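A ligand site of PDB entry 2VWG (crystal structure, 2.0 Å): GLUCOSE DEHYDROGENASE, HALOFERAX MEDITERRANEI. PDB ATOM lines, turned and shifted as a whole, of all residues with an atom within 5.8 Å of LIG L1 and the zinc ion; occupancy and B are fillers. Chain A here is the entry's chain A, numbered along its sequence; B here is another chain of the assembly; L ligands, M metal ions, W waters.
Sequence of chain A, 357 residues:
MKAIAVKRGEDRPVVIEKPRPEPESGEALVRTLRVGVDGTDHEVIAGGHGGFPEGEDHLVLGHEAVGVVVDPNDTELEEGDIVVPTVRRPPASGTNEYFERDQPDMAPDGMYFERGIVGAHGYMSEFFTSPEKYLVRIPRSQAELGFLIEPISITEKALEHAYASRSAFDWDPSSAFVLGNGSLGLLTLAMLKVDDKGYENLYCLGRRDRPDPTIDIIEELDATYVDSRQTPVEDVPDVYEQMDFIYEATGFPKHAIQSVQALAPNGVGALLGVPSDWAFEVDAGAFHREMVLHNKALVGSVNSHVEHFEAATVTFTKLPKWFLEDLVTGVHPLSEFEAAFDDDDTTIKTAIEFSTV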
ATOM      1  N   ASP A  38       7.257 -25.439  14.542  1.00  0.00           N
ATOM      2  CA  ASP A  38       6.778 -26.270  15.667  1.00  0.00           C
ATOM      3  C   ASP A  38       6.315 -27.647  15.195  1.00  0.00           C
ATOM      4  O   ASP A  38       6.423 -27.976  14.012  1.00  0.00           O
ATOM      5  CB  ASP A  38       5.699 -25.544  16.497  1.00  0.00           C
ATOM      6  CG  ASP A  38       4.338 -25.493  15.810  1.00  0.00           C
ATOM      7  OD1 ASP A  38       4.230 -25.898  14.646  1.00  0.00           O
ATOM      8  OD2 ASP A  38       3.375 -25.024  16.433  1.00  0.00           O
ATOM      9  N   THR A  40       3.354 -28.785  14.796  1.00  0.00           N
ATOM     10  CA  THR A  40       2.283 -28.708  13.798  1.00  0.00           C
ATOM     11  C   THR A  40       2.868 -28.620  12.386  1.00  0.00           C
ATOM     12  O   THR A  40       2.359 -29.263  11.464  1.00  0.00           O
ATOM     13  CB  THR A  40       1.357 -27.515  14.055  1.00  0.00           C
ATOM     14  OG1 THR A  40       0.810 -27.606  15.392  1.00  0.00           O
ATOM     15  CG2 THR A  40       0.230 -27.489  13.017  1.00  0.00           C
ATOM     16  N   ASP A  41       3.924 -27.825  12.206  1.00  0.00           N
ATOM     17  CA  ASP A  41       4.569 -27.700  10.886  1.00  0.00           C
ATOM     18  C   ASP A  41       5.108 -29.046  10.365  1.00  0.00           C
ATOM     19  O   ASP A  41       5.042 -29.331   9.172  1.00  0.00           O
ATOM     20  CB  ASP A  41       5.730 -26.704  10.921  1.00  0.00           C
ATOM     21  CG  ASP A  41       5.272 -25.281  11.228  1.00  0.00           C
ATOM     22  OD1 ASP A  41       4.262 -24.852  10.665  1.00  0.00           O
ATOM     23  OD2 ASP A  41       5.913 -24.632  12.067  1.00  0.00           O
ATOM     24  N   HIS A  49      -1.835 -33.389   9.006  1.00  0.00           N
ATOM     25  CA  HIS A  49      -2.725 -32.274   9.376  1.00  0.00           C
ATOM     26  C   HIS A  49      -2.666 -31.175   8.299  1.00  0.00           C
ATOM     27  O   HIS A  49      -1.647 -30.998   7.632  1.00  0.00           O
ATOM     28  CB  HIS A  49      -2.315 -31.702  10.745  1.00  0.00           C
ATOM     29  CG  HIS A  49      -3.199 -30.606  11.254  1.00  0.00           C
ATOM     30  ND1 HIS A  49      -4.532 -30.790  11.561  1.00  0.00           N
ATOM     31  CD2 HIS A  49      -2.932 -29.309  11.544  1.00  0.00           C
ATOM     32  CE1 HIS A  49      -5.052 -29.659  11.997  1.00  0.00           C
ATOM     33  NE2 HIS A  49      -4.099 -28.732  11.993  1.00  0.00           N
ATOM     34  N   HIS A  63       3.447 -20.399  10.519  1.00  0.00           N
ATOM     35  CA  HIS A  63       2.306 -19.711  11.112  1.00  0.00           C
ATOM     36  C   HIS A  63       2.680 -18.882  12.336  1.00  0.00           C
ATOM     37  O   HIS A  63       1.834 -18.207  12.901  1.00  0.00           O
ATOM     38  CB  HIS A  63       1.204 -20.732  11.425  1.00  0.00           C
ATOM     39  CG  HIS A  63       1.611 -21.757  12.433  1.00  0.00           C
ATOM     40  ND1 HIS A  63       2.233 -22.935  12.076  1.00  0.00           N
ATOM     41  CD2 HIS A  63       1.547 -21.754  13.788  1.00  0.00           C
ATOM     42  CE1 HIS A  63       2.509 -23.621  13.179  1.00  0.00           C
ATOM     43  NE2 HIS A  63       2.099 -22.936  14.214  1.00  0.00           N
ATOM     44  N   GLU A  64       3.958 -18.931  12.738  1.00  0.00           N
ATOM     45  CA  GLU A  64       4.487 -18.232  13.886  1.00  0.00           C
ATOM     46  C   GLU A  64       5.485 -17.183  13.369  1.00  0.00           C
ATOM     47  O   GLU A  64       6.660 -17.487  13.195  1.00  0.00           O
ATOM     48  CB  GLU A  64       5.250 -19.179  14.810  1.00  0.00           C
ATOM     49  CG  GLU A  64       4.474 -20.400  15.334  1.00  0.00           C
ATOM     50  CD  GLU A  64       5.342 -21.290  16.198  1.00  0.00           C
ATOM     51  OE1 GLU A  64       6.584 -21.080  16.264  1.00  0.00           O
ATOM     52  OE2 GLU A  64       4.792 -22.216  16.832  1.00  0.00           O
ATOM     53  N   VAL A  87      -3.454 -16.161  12.689  1.00  0.00           N
ATOM     54  CA  VAL A  87      -3.342 -17.277  11.786  1.00  0.00           C
ATOM     55  C   VAL A  87      -4.600 -17.506  10.927  1.00  0.00           C
ATOM     56  O   VAL A  87      -4.486 -17.870   9.758  1.00  0.00           O
ATOM     57  CB  VAL A  87      -2.953 -18.534  12.554  1.00  0.00           C
ATOM     58  CG1 VAL A  87      -2.959 -19.786  11.646  1.00  0.00           C
ATOM     59  CG2 VAL A  87      -1.564 -18.316  13.204  1.00  0.00           C
ATOM     60  N   ARG A  88      -5.785 -17.258  11.476  1.00  0.00           N
ATOM     61  CA  ARG A  88      -7.011 -17.570  10.743  1.00  0.00           C
ATOM     62  C   ARG A  88      -7.490 -16.445   9.822  1.00  0.00           C
ATOM     63  O   ARG A  88      -7.402 -15.269  10.161  1.00  0.00           O
ATOM     64  CB  ARG A  88      -8.121 -18.043  11.685  1.00  0.00           C
ATOM     65  CG  ARG A  88      -7.941 -19.472  12.035  1.00  0.00           C
ATOM     66  CD  ARG A  88      -9.014 -20.004  12.914  1.00  0.00           C
ATOM     67  NE  ARG A  88      -8.721 -21.401  13.262  1.00  0.00           N
ATOM     68  CZ  ARG A  88      -9.562 -22.213  13.898  1.00  0.00           C
ATOM     69  NH1 ARG A  88     -10.745 -21.772  14.293  1.00  0.00           N
ATOM     70  NH2 ARG A  88      -9.209 -23.464  14.146  1.00  0.00           N
ATOM     71  N   GLU A 114      -6.306 -21.430   7.737  1.00  0.00           N
ATOM     72  CA  GLU A 114      -5.170 -21.135   8.621  1.00  0.00           C
ATOM     73  C   GLU A 114      -3.920 -20.984   7.784  1.00  0.00           C
ATOM     74  O   GLU A 114      -3.468 -21.927   7.127  1.00  0.00           O
ATOM     75  CB  GLU A 114      -4.978 -22.247   9.645  1.00  0.00           C
ATOM     76  CG  GLU A 114      -5.991 -22.189  10.748  1.00  0.00           C
ATOM     77  CD  GLU A 114      -5.908 -23.345  11.747  1.00  0.00           C
ATOM     78  OE1 GLU A 114      -5.211 -24.350  11.535  1.00  0.00           O
ATOM     79  OE2 GLU A 114      -6.589 -23.225  12.775  1.00  0.00           O
ATOM     80  N   ILE A 117      -1.048 -23.652   7.254  1.00  0.00           N
ATOM     81  CA  ILE A 117      -1.541 -24.908   7.785  1.00  0.00           C
ATOM     82  C   ILE A 117      -2.654 -25.480   6.891  1.00  0.00           C
ATOM     83  O   ILE A 117      -2.536 -26.593   6.389  1.00  0.00           O
ATOM     84  CB  ILE A 117      -2.062 -24.760   9.225  1.00  0.00           C
ATOM     85  CG1 ILE A 117      -0.993 -24.144  10.126  1.00  0.00           C
ATOM     86  CG2 ILE A 117      -2.470 -26.137   9.793  1.00  0.00           C
ATOM     87  CD1 ILE A 117      -1.449 -23.920  11.563  1.00  0.00           C
ATOM     88  N   GLU A 150       2.919 -16.047  19.062  1.00  0.00           N
ATOM     89  CA  GLU A 150       1.823 -16.907  18.630  1.00  0.00           C
ATOM     90  C   GLU A 150       1.645 -18.147  19.532  1.00  0.00           C
ATOM     91  O   GLU A 150       0.537 -18.393  20.014  1.00  0.00           O
ATOM     92  CB  GLU A 150       1.936 -17.263  17.137  1.00  0.00           C
ATOM     93  CG  GLU A 150       0.689 -17.905  16.550  1.00  0.00           C
ATOM     94  CD  GLU A 150       0.621 -19.406  16.732  1.00  0.00           C
ATOM     95  OE1 GLU A 150       1.636 -20.034  17.108  1.00  0.00           O
ATOM     96  OE2 GLU A 150      -0.472 -19.981  16.490  1.00  0.00           O
ATOM     97  N   PRO A 151       2.711 -18.933  19.752  1.00  0.00           N
ATOM     98  CA  PRO A 151       2.542 -20.088  20.656  1.00  0.00           C
ATOM     99  C   PRO A 151       2.167 -19.722  22.094  1.00  0.00           C
ATOM    100  O   PRO A 151       1.409 -20.451  22.719  1.00  0.00           O
ATOM    101  CB  PRO A 151       3.892 -20.809  20.575  1.00  0.00           C
ATOM    102  CG  PRO A 151       4.814 -19.878  19.868  1.00  0.00           C
ATOM    103  CD  PRO A 151       4.040 -18.904  19.101  1.00  0.00           C
ATOM    104  N   ILE A 154      -1.562 -19.247  22.208  1.00  0.00           N
ATOM    105  CA  ILE A 154      -2.269 -20.529  22.250  1.00  0.00           C
ATOM    106  C   ILE A 154      -2.594 -20.917  23.695  1.00  0.00           C
ATOM    107  O   ILE A 154      -3.734 -21.263  24.025  1.00  0.00           O
ATOM    108  CB  ILE A 154      -1.424 -21.666  21.561  1.00  0.00           C
ATOM    109  CG1 ILE A 154      -1.300 -21.413  20.049  1.00  0.00           C
ATOM    110  CG2 ILE A 154      -2.006 -23.096  21.829  1.00  0.00           C
ATOM    111  CD1 ILE A 154      -2.615 -21.269  19.325  1.00  0.00           C
ATOM    112  N   VAL A 274      -2.978 -32.201  18.767  1.00  0.00           N
ATOM    113  CA  VAL A 274      -3.661 -32.586  17.529  1.00  0.00           C
ATOM    114  C   VAL A 274      -3.274 -34.042  17.294  1.00  0.00           C
ATOM    115  O   VAL A 274      -2.144 -34.337  16.907  1.00  0.00           O
ATOM    116  CB  VAL A 274      -3.225 -31.716  16.353  1.00  0.00           C
ATOM    117  CG1 VAL A 274      -3.942 -32.149  15.077  1.00  0.00           C
ATOM    118  CG2 VAL A 274      -3.506 -30.242  16.666  1.00  0.00           C
ATOM    119  N   VAL A 302      -8.228 -24.602  20.507  1.00  0.00           N
ATOM    120  CA  VAL A 302      -7.422 -24.489  19.299  1.00  0.00           C
ATOM    121  C   VAL A 302      -7.350 -23.034  18.870  1.00  0.00           C
ATOM    122  O   VAL A 302      -8.304 -22.265  19.077  1.00  0.00           O
ATOM    123  CB  VAL A 302      -7.966 -25.402  18.149  1.00  0.00           C
ATOM    124  CG1 VAL A 302      -9.335 -24.904  17.633  1.00  0.00           C
ATOM    125  CG2 VAL A 302      -6.934 -25.499  17.006  1.00  0.00           C
ATOM    126  N   ASN A 303      -6.201 -22.644  18.319  1.00  0.00           N
ATOM    127  CA  ASN A 303      -6.028 -21.327  17.737  1.00  0.00           C
ATOM    128  C   ASN A 303      -6.077 -20.272  18.857  1.00  0.00           C
ATOM    129  O   ASN A 303      -5.944 -20.596  20.043  1.00  0.00           O
ATOM    130  CB  ASN A 303      -7.070 -21.112  16.608  1.00  0.00           C
ATOM    131  CG  ASN A 303      -6.719 -19.951  15.687  1.00  0.00           C
ATOM    132  OD1 ASN A 303      -7.447 -18.973  15.639  1.00  0.00           O
ATOM    133  ND2 ASN A 303      -5.621 -20.073  14.935  1.00  0.00           N
ATOM    134  N   SER A 304      -6.231 -19.018  18.471  1.00  0.00           N
ATOM    135  CA  SER A 304      -6.209 -17.897  19.403  1.00  0.00           C
ATOM    136  C   SER A 304      -6.524 -16.655  18.586  1.00  0.00           C
ATOM    137  O   SER A 304      -6.447 -16.681  17.355  1.00  0.00           O
ATOM    138  CB  SER A 304      -4.836 -17.759  20.066  1.00  0.00           C
ATOM    139  OG  SER A 304      -3.794 -17.643  19.107  1.00  0.00           O
ATOM    140  N   LYS A 349      13.203 -25.284  20.202  1.00  0.00           N
ATOM    141  CA  LYS A 349      12.498 -24.334  19.341  1.00  0.00           C
ATOM    142  C   LYS A 349      13.470 -23.761  18.327  1.00  0.00           C
ATOM    143  O   LYS A 349      14.533 -23.257  18.692  1.00  0.00           O
ATOM    144  CB  LYS A 349      11.886 -23.195  20.136  1.00  0.00           C
ATOM    145  CG  LYS A 349      10.995 -22.278  19.344  1.00  0.00           C
ATOM    146  CD  LYS A 349       9.703 -22.980  19.013  1.00  0.00           C
ATOM    147  CE  LYS A 349       8.811 -22.147  18.183  1.00  0.00           C
ATOM    148  NZ  LYS A 349       7.609 -22.933  17.793  1.00  0.00           N
ATOM    149  N   LEU B 293     -10.026 -29.686  18.216  1.00  0.00           N
ATOM    150  CA  LEU B 293     -10.226 -28.924  16.970  1.00  0.00           C
ATOM    151  C   LEU B 293     -11.564 -28.195  16.922  1.00  0.00           C
ATOM    152  O   LEU B 293     -11.725 -27.246  16.155  1.00  0.00           O
ATOM    153  CB  LEU B 293     -10.052 -29.830  15.742  1.00  0.00           C
ATOM    154  CG  LEU B 293      -8.624 -30.346  15.509  1.00  0.00           C
ATOM    155  CD1 LEU B 293      -8.543 -31.160  14.232  1.00  0.00           C
ATOM    156  CD2 LEU B 293      -7.614 -29.217  15.463  1.00  0.00           C
HETATM  157  C1  LIG L   1      -1.202 -24.572  15.526  1.00  0.00           C
HETATM  158  C2  LIG L   1      -1.463 -23.109  15.524  1.00  0.00           C
HETATM  159  O1  LIG L   1      -2.212 -25.514  15.216  1.00  0.00           O
HETATM  160  O2  LIG L   1      -0.072 -24.982  15.767  1.00  0.00           O
HETATM  161  O3  LIG L   1      -0.744 -22.506  16.575  1.00  0.00           O
HETATM  162  C3  LIG L   1      -2.935 -22.749  15.645  1.00  0.00           C
HETATM  163  O4  LIG L   1      -3.118 -21.417  15.189  1.00  0.00           O
HETATM  164  C4  LIG L   1      -3.804 -23.675  14.814  1.00  0.00           C
HETATM  165  O5  LIG L   1      -5.144 -23.295  15.024  1.00  0.00           O
HETATM  166  C5  LIG L   1      -3.578 -25.123  15.261  1.00  0.00           C
HETATM  167  C6  LIG L   1      -4.402 -26.101  14.420  1.00  0.00           C
HETATM  168  O6  LIG L   1      -3.981 -26.043  13.079  1.00  0.00           O
HETATM  169  P1  LG2 L   2       6.331 -31.365  19.688  1.00  0.00           P
HETATM  170  O1  LG2 L   2       7.521 -30.486  19.597  1.00  0.00           O
HETATM  171  O2  LG2 L   2       6.211 -32.516  18.796  1.00  0.00           O
HETATM  172  O3  LG2 L   2       6.243 -31.828  21.219  1.00  0.00           O
HETATM  173  C1  LG2 L   2       5.528 -32.976  21.561  1.00  0.00           C
HETATM  174  C2  LG2 L   2       6.269 -33.629  22.700  1.00  0.00           C
HETATM  175  O4  LG2 L   2       5.453 -34.589  23.318  1.00  0.00           O
HETATM  176  C3  LG2 L   2       7.556 -34.311  22.219  1.00  0.00           C
HETATM  177  O5  LG2 L   2       8.685 -33.744  22.846  1.00  0.00           O
HETATM  178  C4  LG2 L   2       7.338 -35.756  22.628  1.00  0.00           C
HETATM  179  O6  LG2 L   2       8.494 -36.351  23.124  1.00  0.00           O
HETATM  180  C5  LG2 L   2       6.262 -35.661  23.712  1.00  0.00           C
HETATM  181  N1  LG2 L   2       5.516 -36.925  23.811  1.00  0.00           N
HETATM  182  C6  LG2 L   2       4.764 -37.536  22.840  1.00  0.00           C
HETATM  183  N2  LG2 L   2       4.253 -38.675  23.358  1.00  0.00           N
HETATM  184  C7  LG2 L   2       4.674 -38.792  24.630  1.00  0.00           C
HETATM  185  C8  LG2 L   2       4.456 -39.765  25.605  1.00  0.00           C
HETATM  186  N3  LG2 L   2       3.715 -40.820  25.349  1.00  0.00           N
HETATM  187  N4  LG2 L   2       5.033 -39.598  26.837  1.00  0.00           N
HETATM  188  C9  LG2 L   2       5.803 -38.483  27.125  1.00  0.00           C
HETATM  189  N5  LG2 L   2       6.015 -37.532  26.149  1.00  0.00           N
HETATM  190  C10 LG2 L   2       5.453 -37.690  24.933  1.00  0.00           C
HETATM  191  O7  LG2 L   2       5.017 -30.464  19.495  1.00  0.00           O
HETATM  192  P2  LG2 L   2       4.709 -28.981  20.024  1.00  0.00           P
HETATM  193  O8  LG2 L   2       5.241 -28.769  21.400  1.00  0.00           O
HETATM  194  O9  LG2 L   2       5.025 -27.990  18.974  1.00  0.00           O
HETATM  195  O10 LG2 L   2       3.109 -29.156  20.123  1.00  0.00           O
HETATM  196  C11 LG2 L   2       2.574 -30.158  20.959  1.00  0.00           C
HETATM  197  C12 LG2 L   2       1.206 -30.591  20.448  1.00  0.00           C
HETATM  198  O11 LG2 L   2       0.310 -29.491  20.492  1.00  0.00           O
HETATM  199  C13 LG2 L   2       1.218 -31.073  19.000  1.00  0.00           C
HETATM  200  O12 LG2 L   2       0.261 -32.114  18.882  1.00  0.00           O
HETATM  201  C14 LG2 L   2       0.764 -29.860  18.231  1.00  0.00           C
HETATM  202  O13 LG2 L   2       0.194 -30.187  17.008  1.00  0.00           O
HETATM  203  C15 LG2 L   2      -0.261 -29.285  19.218  1.00  0.00           C
HETATM  204  N6  LG2 L   2      -0.554 -27.857  19.057  1.00  0.00           N
HETATM  205  C16 LG2 L   2      -1.863 -27.485  19.093  1.00  0.00           C
HETATM  206  C17 LG2 L   2      -2.217 -26.163  19.006  1.00  0.00           C
HETATM  207  C18 LG2 L   2      -3.638 -25.780  19.266  1.00  0.00           C
HETATM  208  O14 LG2 L   2      -4.082 -24.598  18.722  1.00  0.00           O
HETATM  209  N7  LG2 L   2      -4.431 -26.608  19.955  1.00  0.00           N
HETATM  210  C19 LG2 L   2      -1.240 -25.197  18.841  1.00  0.00           C
HETATM  211  C20 LG2 L   2       0.102 -25.588  18.819  1.00  0.00           C
HETATM  212  C21 LG2 L   2       0.440 -26.931  18.932  1.00  0.00           C
HETATM  213  P3  LG2 L   2       9.545 -37.129  22.162  1.00  0.00           P
HETATM  214  O15 LG2 L   2      10.292 -36.098  21.400  1.00  0.00           O
HETATM  215  O16 LG2 L   2       8.849 -38.073  21.246  1.00  0.00           O
HETATM  216  O17 LG2 L   2      10.462 -37.824  23.154  1.00  0.00           O
HETATM  217 ZN    ZN M   1       2.898 -22.998  16.206  1.00  0.00          ZN
HETATM  218  O   HOH W   1       1.721 -22.387  17.452  1.00  0.00           O
HETATM  219  O   HOH W   2      -3.009 -18.794  16.726  1.00  0.00           O
HETATM  220  O   HOH W   3      -6.959 -26.581  11.899  1.00  0.00           O
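Val 87 touches LIG L1 (CG1 to O4, 3.9 Å).
Ile 117 touches LIG L1.
Ile 154 touches LIG L1.
Val 302 touches LIG L1.
Hydrophobic or aromatic side chains within 4 Å of LIG L1: His 49, His 63, Val 87, Ile 117, Ile 154 and Val 302.
11 residues have an atom within 4 Å of LIG L1: Asp 38, Thr 40, His 49, His 63, Val 87, Glu 114, Ile 117, Glu 150, Ile 154, Val 302 and Asn 303.
N of Thr 40 is in hydrogen-bond range of OD1 of Asp 38, 3.0 Å away.
OE1 of Glu 64 lies within salt-bridge range of NZ of Lys 349, at 2.6 Å.
ND1 of His 63 is in hydrogen-bond range of OD1 of Asp 41 (3.1 Å).
The guanidinium group (NE) of Arg 88 is in salt-bridge range of the side-chain carboxylate (OE2) of Glu 114 (2.8 Å).
The backbone NH (N) of Asp 38 is in hydrogen-bond range of the side-chain carboxylate (OD2) of Asp 41 (2.9 Å).
Merely in contact with the zinc ion: Glu 150 (3.3 Å).
Along chain A the residues within 4 Å of the zinc ion span positions 38 to 150.
The nearest printed residue that does not touch the zinc ion is Lys 349 (5.0 Å).
The zinc ion is bound by water W1 (1.8 Å).
The zinc ion is bound by OD2 of Asp 38 (2.1 Å).
OE2 of Glu 64 binds the zinc ion, at 2.1 Å.
A ring nitrogen (NE2) of His 63 is bound to the zinc ion (2.1 Å).
The side-chain amide nitrogen of Asn 303 is in hydrogen-bond range of an oxygen (O4) of LIG L1, at 2.9 Å.
NE2 of His 63 lies close to O2 of LIG L1 (3.4 Å).
An oxygen (O14) of LG2 L2 lies within hydrogen-bond range of the backbone NH of Asn 303 (2.9 Å).
An oxygen (O6) of LIG L1 lies within hydrogen-bond range of the side-chain carboxylate (OE1) of Glu 114 (2.6 Å).
OG1 of Thr 40 is in hydrogen-bond range of O2 of LIG L1 (2.8 Å).
The backbone NH (N) of Val 274 sits at hydrogen-bond distance from an oxygen (O12) of LG2 L2 (3.2 Å).
OG1 of Thr 40 lies within hydrogen-bond range of O13 of LG2 L2 (3.1 Å).
The side-chain carboxylate (OE2) of Glu 150 is in hydrogen-bond range of an oxygen (O3) of LIG L1, 2.5 Å away.
NE2 of His 49 sits at hydrogen-bond distance from O6 of LIG L1.
Water W1 lies within hydrogen-bond range of an oxygen (O3) of LIG L1 (2.6 Å) and the side-chain carboxylate (OE2) of Glu 150 (3.4 Å).
Water W2 lies within hydrogen-bond range of the side-chain hydroxyl (OG) of Ser 304 (2.8 Å), the side-chain carboxylate (OE2) of Glu 150 (2.8 Å), an oxygen (O4) of LIG L1 (3.0 Å) and the side-chain amide nitrogen (ND2) of Asn 303 (3.4 Å).
Water W3 bridges OE1 of Glu 114 and O6 of LIG L1.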
